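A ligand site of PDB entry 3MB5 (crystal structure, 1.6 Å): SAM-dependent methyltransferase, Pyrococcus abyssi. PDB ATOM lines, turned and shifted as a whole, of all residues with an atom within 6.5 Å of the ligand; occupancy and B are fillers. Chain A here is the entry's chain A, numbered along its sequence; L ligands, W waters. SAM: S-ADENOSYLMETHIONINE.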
ATOM      1  N   MET A  70       8.130  -5.522  19.118  1.00  0.00           N
ATOM      2  CA  MET A  70       7.044  -4.661  19.615  1.00  0.00           C
ATOM      3  C   MET A  70       5.654  -5.154  19.172  1.00  0.00           C
ATOM      4  O   MET A  70       5.521  -5.850  18.160  1.00  0.00           O
ATOM      5  CB  MET A  70       7.244  -3.231  19.088  1.00  0.00           C
ATOM      6  CG  MET A  70       7.192  -3.174  17.571  1.00  0.00           C
ATOM      7  SD  MET A  70       7.424  -1.525  16.862  1.00  0.00           S
ATOM      8  CE  MET A  70       5.888  -0.727  17.400  1.00  0.00           C
ATOM      9  N   PRO A  74      -1.748  -0.279  14.160  1.00  0.00           N
ATOM     10  CA  PRO A  74      -1.761   0.356  12.833  1.00  0.00           C
ATOM     11  C   PRO A  74      -0.437   0.080  12.107  1.00  0.00           C
ATOM     12  O   PRO A  74       0.609  -0.083  12.760  1.00  0.00           O
ATOM     13  CB  PRO A  74      -1.923   1.845  13.125  1.00  0.00           C
ATOM     14  CG  PRO A  74      -1.809   2.006  14.587  1.00  0.00           C
ATOM     15  CD  PRO A  74      -1.933   0.683  15.260  1.00  0.00           C
ATOM     16  N   GLN A  75      -0.500  -0.006  10.778  1.00  0.00           N
ATOM     17  CA  GLN A  75       0.655  -0.326   9.927  1.00  0.00           C
ATOM     18  C   GLN A  75       1.907   0.470  10.300  1.00  0.00           C
ATOM     19  O   GLN A  75       1.869   1.691  10.302  1.00  0.00           O
ATOM     20  CB  GLN A  75       0.335  -0.071   8.457  1.00  0.00           C
ATOM     21  CG  GLN A  75       1.526  -0.352   7.534  1.00  0.00           C
ATOM     22  CD  GLN A  75       1.901  -1.807   7.561  1.00  0.00           C
ATOM     23  OE1 GLN A  75       1.079  -2.671   7.231  1.00  0.00           O
ATOM     24  NE2 GLN A  75       3.133  -2.092   7.978  1.00  0.00           N
ATOM     25  N   ILE A  76       2.975  -0.235  10.652  1.00  0.00           N
ATOM     26  CA  ILE A  76       4.234   0.396  11.050  1.00  0.00           C
ATOM     27  C   ILE A  76       5.024   0.907   9.842  1.00  0.00           C
ATOM     28  O   ILE A  76       4.874   0.390   8.724  1.00  0.00           O
ATOM     29  CB  ILE A  76       5.123  -0.578  11.872  1.00  0.00           C
ATOM     30  CG1 ILE A  76       5.387  -1.851  11.064  1.00  0.00           C
ATOM     31  CG2 ILE A  76       4.483  -0.938  13.208  1.00  0.00           C
ATOM     32  CD1 ILE A  76       6.816  -2.343  11.223  1.00  0.00           C
ATOM     33  N   VAL A  77       5.873   1.908  10.060  1.00  0.00           N
ATOM     34  CA  VAL A  77       6.872   2.312   9.065  1.00  0.00           C
ATOM     35  C   VAL A  77       8.028   1.311   9.149  1.00  0.00           C
ATOM     36  O   VAL A  77       8.572   1.050  10.233  1.00  0.00           O
ATOM     37  CB  VAL A  77       7.390   3.767   9.304  1.00  0.00           C
ATOM     38  CG1 VAL A  77       8.638   4.049   8.483  1.00  0.00           C
ATOM     39  CG2 VAL A  77       6.322   4.793   8.949  1.00  0.00           C
ATOM     40  N   HIS A  78       8.396   0.751   7.982  1.00  0.00           N
ATOM     41  CA  HIS A  78       9.444  -0.241   7.856  1.00  0.00           C
ATOM     42  C   HIS A  78      10.801   0.396   8.212  1.00  0.00           C
ATOM     43  O   HIS A  78      11.046   1.576   7.870  1.00  0.00           O
ATOM     44  CB  HIS A  78       9.430  -0.694   6.391  1.00  0.00           C
ATOM     45  CG  HIS A  78      10.265  -1.902   6.114  1.00  0.00           C
ATOM     46  ND1 HIS A  78      11.631  -1.849   6.022  1.00  0.00           N
ATOM     47  CD2 HIS A  78       9.907  -3.187   5.891  1.00  0.00           C
ATOM     48  CE1 HIS A  78      12.101  -3.063   5.760  1.00  0.00           C
ATOM     49  NE2 HIS A  78      11.077  -3.888   5.673  1.00  0.00           N
ATOM     50  N   GLU A  99       6.194  14.469  15.645  1.00  0.00           N
ATOM     51  CA  GLU A  99       5.777  13.333  14.779  1.00  0.00           C
ATOM     52  C   GLU A  99       4.253  13.204  14.780  1.00  0.00           C
ATOM     53  O   GLU A  99       3.597  13.488  15.787  1.00  0.00           O
ATOM     54  CB  GLU A  99       6.387  12.057  15.371  1.00  0.00           C
ATOM     55  CG  GLU A  99       6.016  10.804  14.542  1.00  0.00           C
ATOM     56  CD  GLU A  99       6.199   9.499  15.256  1.00  0.00           C
ATOM     57  OE1 GLU A  99       6.293   9.428  16.520  1.00  0.00           O
ATOM     58  OE2 GLU A  99       6.233   8.474  14.530  1.00  0.00           O
ATOM     59  N   ALA A 100       3.673  12.760  13.672  1.00  0.00           N
ATOM     60  CA  ALA A 100       2.244  12.368  13.704  1.00  0.00           C
ATOM     61  C   ALA A 100       1.935  11.456  12.542  1.00  0.00           C
ATOM     62  O   ALA A 100       2.535  11.628  11.489  1.00  0.00           O
ATOM     63  CB  ALA A 100       1.349  13.614  13.610  1.00  0.00           C
ATOM     64  N   GLY A 101       1.048  10.467  12.689  1.00  0.00           N
ATOM     65  CA  GLY A 101       0.480  10.031  13.959  1.00  0.00           C
ATOM     66  C   GLY A 101       1.342   8.962  14.605  1.00  0.00           C
ATOM     67  O   GLY A 101       2.086   8.234  13.899  1.00  0.00           O
ATOM     68  N   VAL A 102       1.243   8.845  15.931  1.00  0.00           N
ATOM     69  CA  VAL A 102       2.092   7.862  16.645  1.00  0.00           C
ATOM     70  C   VAL A 102       1.851   6.429  16.150  1.00  0.00           C
ATOM     71  O   VAL A 102       2.804   5.644  16.085  1.00  0.00           O
ATOM     72  CB  VAL A 102       1.953   7.968  18.190  1.00  0.00           C
ATOM     73  CG1 VAL A 102       0.660   7.301  18.684  1.00  0.00           C
ATOM     74  CG2 VAL A 102       3.178   7.376  18.888  1.00  0.00           C
ATOM     75  N   GLY A 103       0.608   6.095  15.800  1.00  0.00           N
ATOM     76  CA  GLY A 103       0.321   4.732  15.287  1.00  0.00           C
ATOM     77  C   GLY A 103       0.659   3.680  16.332  1.00  0.00           C
ATOM     78  O   GLY A 103       0.155   3.730  17.464  1.00  0.00           O
ATOM     79  N   SER A 104       1.515   2.717  15.966  1.00  0.00           N
ATOM     80  CA  SER A 104       1.975   1.698  16.905  1.00  0.00           C
ATOM     81  C   SER A 104       3.213   2.138  17.672  1.00  0.00           C
ATOM     82  O   SER A 104       3.645   1.450  18.589  1.00  0.00           O
ATOM     83  CB  SER A 104       2.317   0.397  16.155  1.00  0.00           C
ATOM     84  OG  SER A 104       1.173  -0.139  15.516  1.00  0.00           O
ATOM     85  N   GLY A 105       3.812   3.257  17.246  1.00  0.00           N
ATOM     86  CA  GLY A 105       5.068   3.738  17.832  1.00  0.00           C
ATOM     87  C   GLY A 105       6.332   3.157  17.232  1.00  0.00           C
ATOM     88  O   GLY A 105       7.400   3.318  17.784  1.00  0.00           O
ATOM     89  N   ALA A 106       6.249   2.511  16.072  1.00  0.00           N
ATOM     90  CA  ALA A 106       7.472   1.928  15.484  1.00  0.00           C
ATOM     91  C   ALA A 106       8.453   3.011  15.022  1.00  0.00           C
ATOM     92  O   ALA A 106       9.634   2.977  15.380  1.00  0.00           O
ATOM     93  CB  ALA A 106       7.136   1.015  14.330  1.00  0.00           C
ATOM     94  N   LEU A 107       7.969   3.948  14.237  1.00  0.00           N
ATOM     95  CA  LEU A 107       8.803   5.075  13.832  1.00  0.00           C
ATOM     96  C   LEU A 107       9.237   5.876  15.074  1.00  0.00           C
ATOM     97  O   LEU A 107      10.370   6.323  15.147  1.00  0.00           O
ATOM     98  CB  LEU A 107       8.052   5.913  12.782  1.00  0.00           C
ATOM     99  CG  LEU A 107       8.833   7.126  12.264  1.00  0.00           C
ATOM    100  CD1 LEU A 107      10.211   6.797  11.636  1.00  0.00           C
ATOM    101  CD2 LEU A 107       7.954   7.856  11.264  1.00  0.00           C
ATOM    102  N   THR A 108       8.322   6.040  16.037  1.00  0.00           N
ATOM    103  CA  THR A 108       8.627   6.761  17.282  1.00  0.00           C
ATOM    104  C   THR A 108       9.811   6.117  17.980  1.00  0.00           C
ATOM    105  O   THR A 108      10.713   6.833  18.430  1.00  0.00           O
ATOM    106  CB  THR A 108       7.447   6.737  18.243  1.00  0.00           C
ATOM    107  OG1 THR A 108       6.254   7.097  17.547  1.00  0.00           O
ATOM    108  CG2 THR A 108       7.668   7.730  19.395  1.00  0.00           C
ATOM    109  N   TYR A 124       1.862  13.280  17.951  1.00  0.00           N
ATOM    110  CA  TYR A 124       0.421  13.560  17.943  1.00  0.00           C
ATOM    111  C   TYR A 124      -0.362  12.337  17.521  1.00  0.00           C
ATOM    112  O   TYR A 124       0.122  11.546  16.702  1.00  0.00           O
ATOM    113  CB  TYR A 124       0.105  14.710  16.985  1.00  0.00           C
ATOM    114  CG  TYR A 124       0.478  16.101  17.495  1.00  0.00           C
ATOM    115  CD1 TYR A 124      -0.498  17.099  17.565  1.00  0.00           C
ATOM    116  CD2 TYR A 124       1.790  16.426  17.852  1.00  0.00           C
ATOM    117  CE1 TYR A 124      -0.175  18.374  18.016  1.00  0.00           C
ATOM    118  CE2 TYR A 124       2.134  17.713  18.325  1.00  0.00           C
ATOM    119  CZ  TYR A 124       1.133  18.679  18.382  1.00  0.00           C
ATOM    120  OH  TYR A 124       1.448  19.943  18.828  1.00  0.00           O
ATOM    121  N   GLU A 125      -1.563  12.141  18.067  1.00  0.00           N
ATOM    122  CA  GLU A 125      -2.381  10.975  17.709  1.00  0.00           C
ATOM    123  C   GLU A 125      -3.837  11.294  18.026  1.00  0.00           C
ATOM    124  O   GLU A 125      -4.114  11.848  19.080  1.00  0.00           O
ATOM    125  CB  GLU A 125      -1.914   9.725  18.465  1.00  0.00           C
ATOM    126  CG  GLU A 125      -2.769   8.470  18.190  1.00  0.00           C
ATOM    127  CD  GLU A 125      -2.886   8.128  16.717  1.00  0.00           C
ATOM    128  OE1 GLU A 125      -3.991   8.207  16.150  1.00  0.00           O
ATOM    129  OE2 GLU A 125      -1.846   7.793  16.073  1.00  0.00           O
ATOM    130  N   ILE A 126      -4.715  10.988  17.101  1.00  0.00           N
ATOM    131  CA  ILE A 126      -6.150  11.215  17.350  1.00  0.00           C
ATOM    132  C   ILE A 126      -6.879   9.990  17.893  1.00  0.00           C
ATOM    133  O   ILE A 126      -7.903  10.140  18.588  1.00  0.00           O
ATOM    134  CB  ILE A 126      -6.891  11.746  16.115  1.00  0.00           C
ATOM    135  CG1 ILE A 126      -6.774  10.774  14.938  1.00  0.00           C
ATOM    136  CG2 ILE A 126      -6.421  13.164  15.822  1.00  0.00           C
ATOM    137  CD1 ILE A 126      -7.510  11.215  13.684  1.00  0.00           C
ATOM    138  N   ARG A 127      -6.383   8.788  17.573  1.00  0.00           N
ATOM    139  CA  ARG A 127      -7.006   7.546  18.048  1.00  0.00           C
ATOM    140  C   ARG A 127      -6.461   7.180  19.414  1.00  0.00           C
ATOM    141  O   ARG A 127      -5.300   6.833  19.563  1.00  0.00           O
ATOM    142  CB  ARG A 127      -6.767   6.388  17.074  1.00  0.00           C
ATOM    143  CG  ARG A 127      -7.534   6.481  15.765  1.00  0.00           C
ATOM    144  CD  ARG A 127      -8.878   5.809  15.792  1.00  0.00           C
ATOM    145  NE  ARG A 127      -8.852   4.397  16.213  1.00  0.00           N
ATOM    146  CZ  ARG A 127      -9.050   3.349  15.427  1.00  0.00           C
ATOM    147  NH1 ARG A 127      -9.248   3.480  14.122  1.00  0.00           N
ATOM    148  NH2 ARG A 127      -9.053   2.134  15.974  1.00  0.00           N
ATOM    149  N   PHE A 130      -5.074   3.564  19.716  1.00  0.00           N
ATOM    150  CA  PHE A 130      -3.704   3.454  19.142  1.00  0.00           C
ATOM    151  C   PHE A 130      -2.693   4.134  20.048  1.00  0.00           C
ATOM    152  O   PHE A 130      -1.599   3.596  20.265  1.00  0.00           O
ATOM    153  CB  PHE A 130      -3.629   4.064  17.733  1.00  0.00           C
ATOM    154  CG  PHE A 130      -4.462   3.354  16.676  1.00  0.00           C
ATOM    155  CD1 PHE A 130      -4.647   3.973  15.438  1.00  0.00           C
ATOM    156  CD2 PHE A 130      -5.069   2.112  16.887  1.00  0.00           C
ATOM    157  CE1 PHE A 130      -5.398   3.370  14.425  1.00  0.00           C
ATOM    158  CE2 PHE A 130      -5.820   1.492  15.870  1.00  0.00           C
ATOM    159  CZ  PHE A 130      -5.983   2.139  14.636  1.00  0.00           C
ATOM    160  N   ALA A 131      -3.020   5.323  20.584  1.00  0.00           N
ATOM    161  CA  ALA A 131      -2.098   6.005  21.492  1.00  0.00           C
ATOM    162  C   ALA A 131      -1.737   5.189  22.721  1.00  0.00           C
ATOM    163  O   ALA A 131      -0.577   5.184  23.162  1.00  0.00           O
ATOM    164  CB  ALA A 131      -2.658   7.390  21.897  1.00  0.00           C
ATOM    165  N   LYS A 150       0.627  13.461  22.427  1.00  0.00           N
ATOM    166  CA  LYS A 150      -0.464  14.430  22.530  1.00  0.00           C
ATOM    167  C   LYS A 150      -1.675  13.900  21.817  1.00  0.00           C
ATOM    168  O   LYS A 150      -1.619  13.572  20.627  1.00  0.00           O
ATOM    169  CB  LYS A 150      -0.071  15.792  21.945  1.00  0.00           C
ATOM    170  CG  LYS A 150       0.999  16.521  22.735  1.00  0.00           C
ATOM    171  CD  LYS A 150       1.058  17.956  22.258  1.00  0.00           C
ATOM    172  CE  LYS A 150       1.696  18.821  23.302  1.00  0.00           C
ATOM    173  NZ  LYS A 150       1.733  20.228  22.820  1.00  0.00           N
ATOM    174  N   LYS A 152      -4.189  14.965  20.097  1.00  0.00           N
ATOM    175  CA  LYS A 152      -4.605  16.169  19.380  1.00  0.00           C
ATOM    176  C   LYS A 152      -4.551  15.880  17.893  1.00  0.00           C
ATOM    177  O   LYS A 152      -3.696  15.117  17.430  1.00  0.00           O
ATOM    178  CB  LYS A 152      -3.682  17.337  19.719  1.00  0.00           C
ATOM    179  CG  LYS A 152      -3.680  17.776  21.194  1.00  0.00           C
ATOM    180  CD  LYS A 152      -4.849  18.724  21.474  1.00  0.00           C
ATOM    181  CE  LYS A 152      -4.846  19.243  22.915  1.00  0.00           C
ATOM    182  NZ  LYS A 152      -3.519  19.785  23.353  1.00  0.00           N
ATOM    183  N   ASP A 153      -5.448  16.512  17.164  1.00  0.00           N
ATOM    184  CA  ASP A 153      -5.476  16.460  15.710  1.00  0.00           C
ATOM    185  C   ASP A 153      -4.442  17.459  15.190  1.00  0.00           C
ATOM    186  O   ASP A 153      -4.620  18.673  15.291  1.00  0.00           O
ATOM    187  CB  ASP A 153      -6.887  16.871  15.255  1.00  0.00           C
ATOM    188  CG  ASP A 153      -7.051  16.869  13.750  1.00  0.00           C
ATOM    189  OD1 ASP A 153      -8.215  16.917  13.303  1.00  0.00           O
ATOM    190  OD2 ASP A 153      -6.034  16.866  13.003  1.00  0.00           O
ATOM    191  N   ILE A 154      -3.337  16.971  14.618  1.00  0.00           N
ATOM    192  CA  ILE A 154      -2.268  17.875  14.175  1.00  0.00           C
ATOM    193  C   ILE A 154      -2.659  18.820  13.034  1.00  0.00           C
ATOM    194  O   ILE A 154      -1.999  19.823  12.798  1.00  0.00           O
ATOM    195  CB  ILE A 154      -0.946  17.068  13.880  1.00  0.00           C
ATOM    196  CG1 ILE A 154       0.256  18.007  13.790  1.00  0.00           C
ATOM    197  CG2 ILE A 154      -1.136  16.248  12.589  1.00  0.00           C
ATOM    198  CD1 ILE A 154       1.649  17.278  13.745  1.00  0.00           C
ATOM    199  N   TYR A 155      -3.735  18.491  12.309  1.00  0.00           N
ATOM    200  CA  TYR A 155      -4.241  19.346  11.239  1.00  0.00           C
ATOM    201  C   TYR A 155      -4.732  20.671  11.818  1.00  0.00           C
ATOM    202  O   TYR A 155      -4.850  21.637  11.075  1.00  0.00           O
ATOM    203  CB  TYR A 155      -5.396  18.690  10.474  1.00  0.00           C
ATOM    204  CG  TYR A 155      -5.071  17.387   9.764  1.00  0.00           C
ATOM    205  CD1 TYR A 155      -6.083  16.497   9.465  1.00  0.00           C
ATOM    206  CD2 TYR A 155      -3.759  17.062   9.411  1.00  0.00           C
ATOM    207  CE1 TYR A 155      -5.824  15.292   8.798  1.00  0.00           C
ATOM    208  CE2 TYR A 155      -3.486  15.875   8.744  1.00  0.00           C
ATOM    209  CZ  TYR A 155      -4.511  15.001   8.453  1.00  0.00           C
ATOM    210  OH  TYR A 155      -4.235  13.817   7.794  1.00  0.00           O
ATOM    211  N   GLU A 156      -5.007  20.684  13.116  1.00  0.00           N
ATOM    212  CA  GLU A 156      -5.498  21.902  13.775  1.00  0.00           C
ATOM    213  C   GLU A 156      -4.376  22.803  14.274  1.00  0.00           C
ATOM    214  O   GLU A 156      -4.627  23.947  14.662  1.00  0.00           O
ATOM    215  CB  GLU A 156      -6.437  21.521  14.924  1.00  0.00           C
ATOM    216  CG  GLU A 156      -7.708  20.835  14.430  1.00  0.00           C
ATOM    217  CD  GLU A 156      -8.449  21.654  13.363  1.00  0.00           C
ATOM    218  OE1 GLU A 156      -8.631  21.145  12.239  1.00  0.00           O
ATOM    219  OE2 GLU A 156      -8.833  22.817  13.656  1.00  0.00           O
ATOM    220  N   LEU A 168       6.015  12.985   9.373  1.00  0.00           N
ATOM    221  CA  LEU A 168       4.596  12.606   9.217  1.00  0.00           C
ATOM    222  C   LEU A 168       4.366  11.270   8.552  1.00  0.00           C
ATOM    223  O   LEU A 168       4.992  10.981   7.544  1.00  0.00           O
ATOM    224  CB  LEU A 168       3.816  13.653   8.422  1.00  0.00           C
ATOM    225  CG  LEU A 168       3.947  15.066   8.991  1.00  0.00           C
ATOM    226  CD1 LEU A 168       3.301  16.027   8.016  1.00  0.00           C
ATOM    227  CD2 LEU A 168       3.273  15.181  10.380  1.00  0.00           C
ATOM    228  N   ASP A 169       3.458  10.497   9.130  1.00  0.00           N
ATOM    229  CA  ASP A 169       2.881   9.308   8.511  1.00  0.00           C
ATOM    230  C   ASP A 169       1.407   9.367   8.878  1.00  0.00           C
ATOM    231  O   ASP A 169       0.986   8.841   9.932  1.00  0.00           O
ATOM    232  CB  ASP A 169       3.527   8.061   9.103  1.00  0.00           C
ATOM    233  CG  ASP A 169       2.916   6.757   8.600  1.00  0.00           C
ATOM    234  OD1 ASP A 169       2.112   6.799   7.650  1.00  0.00           O
ATOM    235  OD2 ASP A 169       3.237   5.696   9.192  1.00  0.00           O
ATOM    236  N   LEU A 170       0.663  10.071   8.031  1.00  0.00           N
ATOM    237  CA  LEU A 170      -0.787  10.189   8.163  1.00  0.00           C
ATOM    238  C   LEU A 170      -1.355  10.477   6.782  1.00  0.00           C
ATOM    239  O   LEU A 170      -0.611  10.660   5.818  1.00  0.00           O
ATOM    240  CB  LEU A 170      -1.174  11.248   9.221  1.00  0.00           C
ATOM    241  CG  LEU A 170      -0.334  12.530   9.276  1.00  0.00           C
ATOM    242  CD1 LEU A 170      -0.413  13.344   8.002  1.00  0.00           C
ATOM    243  CD2 LEU A 170      -0.915  13.323  10.459  1.00  0.00           C
ATOM    244  N   PRO A 171      -2.681  10.457   6.646  1.00  0.00           N
ATOM    245  CA  PRO A 171      -3.219  10.446   5.272  1.00  0.00           C
ATOM    246  C   PRO A 171      -3.054  11.730   4.459  1.00  0.00           C
ATOM    247  O   PRO A 171      -2.935  11.672   3.247  1.00  0.00           O
ATOM    248  CB  PRO A 171      -4.713  10.131   5.491  1.00  0.00           C
ATOM    249  CG  PRO A 171      -4.744   9.342   6.774  1.00  0.00           C
ATOM    250  CD  PRO A 171      -3.682   9.987   7.648  1.00  0.00           C
ATOM    251  N   GLN A 172      -3.084  12.883   5.117  1.00  0.00           N
ATOM    252  CA  GLN A 172      -3.097  14.144   4.398  1.00  0.00           C
ATOM    253  C   GLN A 172      -2.016  15.090   4.912  1.00  0.00           C
ATOM    254  O   GLN A 172      -2.287  16.131   5.517  1.00  0.00           O
ATOM    255  CB  GLN A 172      -4.478  14.801   4.548  1.00  0.00           C
ATOM    256  CG  GLN A 172      -5.613  14.000   3.897  1.00  0.00           C
ATOM    257  CD  GLN A 172      -6.956  14.651   4.174  1.00  0.00           C
ATOM    258  OE1 GLN A 172      -7.585  15.188   3.265  1.00  0.00           O
ATOM    259  NE2 GLN A 172      -7.364  14.638   5.419  1.00  0.00           N
ATOM    260  N   VAL A 176      -0.581  19.766   6.980  1.00  0.00           N
ATOM    261  CA  VAL A 176       0.351  20.088   8.063  1.00  0.00           C
ATOM    262  C   VAL A 176       1.457  21.036   7.579  1.00  0.00           C
ATOM    263  O   VAL A 176       2.220  21.559   8.399  1.00  0.00           O
ATOM    264  CB  VAL A 176       0.973  18.781   8.688  1.00  0.00           C
ATOM    265  CG1 VAL A 176       1.794  19.091   9.965  1.00  0.00           C
ATOM    266  CG2 VAL A 176      -0.117  17.778   9.044  1.00  0.00           C
ATOM    267  N   TYR A 193       5.835  10.482   4.890  1.00  0.00           N
ATOM    268  CA  TYR A 193       5.745   9.134   4.294  1.00  0.00           C
ATOM    269  C   TYR A 193       4.320   8.961   3.780  1.00  0.00           C
ATOM    270  O   TYR A 193       3.345   9.192   4.505  1.00  0.00           O
ATOM    271  CB  TYR A 193       6.058   8.119   5.385  1.00  0.00           C
ATOM    272  CG  TYR A 193       5.760   6.688   5.018  1.00  0.00           C
ATOM    273  CD1 TYR A 193       4.503   6.126   5.254  1.00  0.00           C
ATOM    274  CD2 TYR A 193       6.735   5.902   4.385  1.00  0.00           C
ATOM    275  CE1 TYR A 193       4.228   4.807   4.910  1.00  0.00           C
ATOM    276  CE2 TYR A 193       6.484   4.581   4.046  1.00  0.00           C
ATOM    277  CZ  TYR A 193       5.222   4.046   4.294  1.00  0.00           C
ATOM    278  OH  TYR A 193       4.952   2.736   3.990  1.00  0.00           O
HETATM  279  N   SAM L   1       4.362   5.681  11.705  1.00  0.00           N
HETATM  280  CA  SAM L   1       3.559   4.811  12.621  1.00  0.00           C
HETATM  281  C   SAM L   1       4.357   3.602  13.109  1.00  0.00           C
HETATM  282  O   SAM L   1       5.501   3.410  12.656  1.00  0.00           O
HETATM  283  OXT SAM L   1       3.887   2.820  13.938  1.00  0.00           O
HETATM  284  CB  SAM L   1       2.246   4.397  11.954  1.00  0.00           C
HETATM  285  CG  SAM L   1       1.304   5.593  11.771  1.00  0.00           C
HETATM  286  SD  SAM L   1      -0.331   5.071  11.174  1.00  0.00           S
HETATM  287  CE  SAM L   1       0.024   4.578   9.453  1.00  0.00           C
HETATM  288  C5' SAM L   1      -1.155   6.670  10.953  1.00  0.00           C
HETATM  289  C4' SAM L   1      -1.524   7.245  12.316  1.00  0.00           C
HETATM  290  O4' SAM L   1      -1.872   8.607  12.119  1.00  0.00           O
HETATM  291  C3' SAM L   1      -2.770   6.546  12.889  1.00  0.00           C
HETATM  292  O3' SAM L   1      -2.467   6.080  14.197  1.00  0.00           O
HETATM  293  C2' SAM L   1      -3.836   7.642  12.796  1.00  0.00           C
HETATM  294  O2' SAM L   1      -4.813   7.524  13.807  1.00  0.00           O
HETATM  295  C1' SAM L   1      -3.001   8.895  12.954  1.00  0.00           C
HETATM  296  N9  SAM L   1      -3.629  10.123  12.444  1.00  0.00           N
HETATM  297  C8  SAM L   1      -4.340  10.298  11.287  1.00  0.00           C
HETATM  298  N7  SAM L   1      -4.703  11.599  11.176  1.00  0.00           N
HETATM  299  C5  SAM L   1      -4.183  12.255  12.243  1.00  0.00           C
HETATM  300  C6  SAM L   1      -4.253  13.581  12.670  1.00  0.00           C
HETATM  301  N6  SAM L   1      -4.879  14.507  11.952  1.00  0.00           N
HETATM  302  N1  SAM L   1      -3.622  13.933  13.836  1.00  0.00           N
HETATM  303  C2  SAM L   1      -2.964  13.005  14.614  1.00  0.00           C
HETATM  304  N3  SAM L   1      -2.919  11.683  14.226  1.00  0.00           N
HETATM  305  C4  SAM L   1      -3.509  11.333  13.047  1.00  0.00           C
HETATM  306  O   HOH W   1      -6.295   8.150   9.849  1.00  0.00           O
HETATM  307  O   HOH W   2      -3.287   4.059  10.114  1.00  0.00           O
HETATM  308  O   HOH W   3      -7.104  12.063   9.819  1.00  0.00           O
HETATM  309  O   HOH W   4       5.439   5.909  15.004  1.00  0.00           O
HETATM  310  O   HOH W   5       2.663   3.324   7.969  1.00  0.00           O
HETATM  311  O   HOH W   6       4.491   8.272  12.565  1.00  0.00           O
HETATM  312  O   HOH W   7      -7.221   7.593  12.442  1.00  0.00           O
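N of the ligand lies within salt-bridge range of OD2 of Asp 169, 2.8 Å away. OD2 of Asp 153 lies within hydrogen-bond range of N6 of the ligand (2.8 Å). N of Gly 105 sits at hydrogen-bond distance from OXT of the ligand (3.3 Å). N of Ile 126 is in hydrogen-bond range of N3 of the ligand (3.5 Å). N of Ala 106 sits at hydrogen-bond distance from OXT of the ligand, at 3.2 Å. An oxygen (O) of the ligand lies within hydrogen-bond range of the backbone NH of Leu 107 (3.0 Å). O of the ligand sits at hydrogen-bond distance from N of Val 77 (3.0 Å). N of Ser 104 sits at hydrogen-bond distance from OXT of the ligand (3.1 Å). A nitrogen (N1) of the ligand is in hydrogen-bond range of the backbone NH (N) of Ile 154. An oxygen (O2') of the ligand sits at hydrogen-bond distance from the side-chain carboxylate of Glu 125 (2.6 Å). The backbone NH of Gly 103 lies close to an oxygen (O3') of the ligand, at 3.5 Å.
The backbone NH (N) of Gly 101 is in hydrogen-bond range of the backbone carbonyl oxygen (O) of Asp 169. N of Glu 125 sits at hydrogen-bond distance from O of Lys 150 (2.9 Å). N of Gly 103 is in hydrogen-bond range of OE2 of Glu 125. O of Ala 100 is in hydrogen-bond range of N of Asp 169, 2.8 Å away. The side-chain carboxylate (OD2) of Asp 153 lies within hydrogen-bond range of the backbone NH (N) of Tyr 155 (2.9 Å). N of Val 102 lies within hydrogen-bond range of O of Tyr 124 (3.0 Å). N of Lys 152 is in hydrogen-bond range of O of Glu 125. N of Tyr 124 is in hydrogen-bond range of O of Glu 99 (2.8 Å).
Merely in contact with the ligand: Gln 75 (3.2 Å), Phe 130 (3.3 Å), Gly 101 (3.3 Å), Tyr 155 (3.4 Å), Arg 127 (3.5 Å), Lys 152 (3.6 Å), Val 102 (3.6 Å), Ile 76 (3.6 Å), Pro 171 (3.7 Å), Leu 170 (3.9 Å) and Tyr 124 (3.9 Å). Hydrophobic or aromatic side chains that line the ligand: Ile 76, Val 77, Ala 106, Leu 107, Ile 126, Phe 130, Ile 154, Tyr 155, Leu 170 and Pro 171. Within 4 Å of the ligand: Gln 75, Ile 76, Val 77, Gly 101, Val 102, Gly 103, Ser 104, Gly 105, Ala 106, Leu 107, Tyr 124, Glu 125, Ile 126, Arg 127, Phe 130, Lys 152, Asp 153, Ile 154, Tyr 155, Asp 169, Leu 170 and Pro 171.
Water W6 lies within hydrogen-bond range of OE2 of Glu 99 (2.6 Å), N of the ligand (2.7 Å) and O of Gly 101 (2.8 Å). Water W4 lies within hydrogen-bond range of OE2 of Glu 99, O of Val 102, OG1 of Thr 108, N of Leu 107 and O of the ligand. Water W5 lies within hydrogen-bond range of the side-chain carboxylate of Asp 169 (2.7 Å) and the backbone carbonyl oxygen of Gln 75 (3.0 Å).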
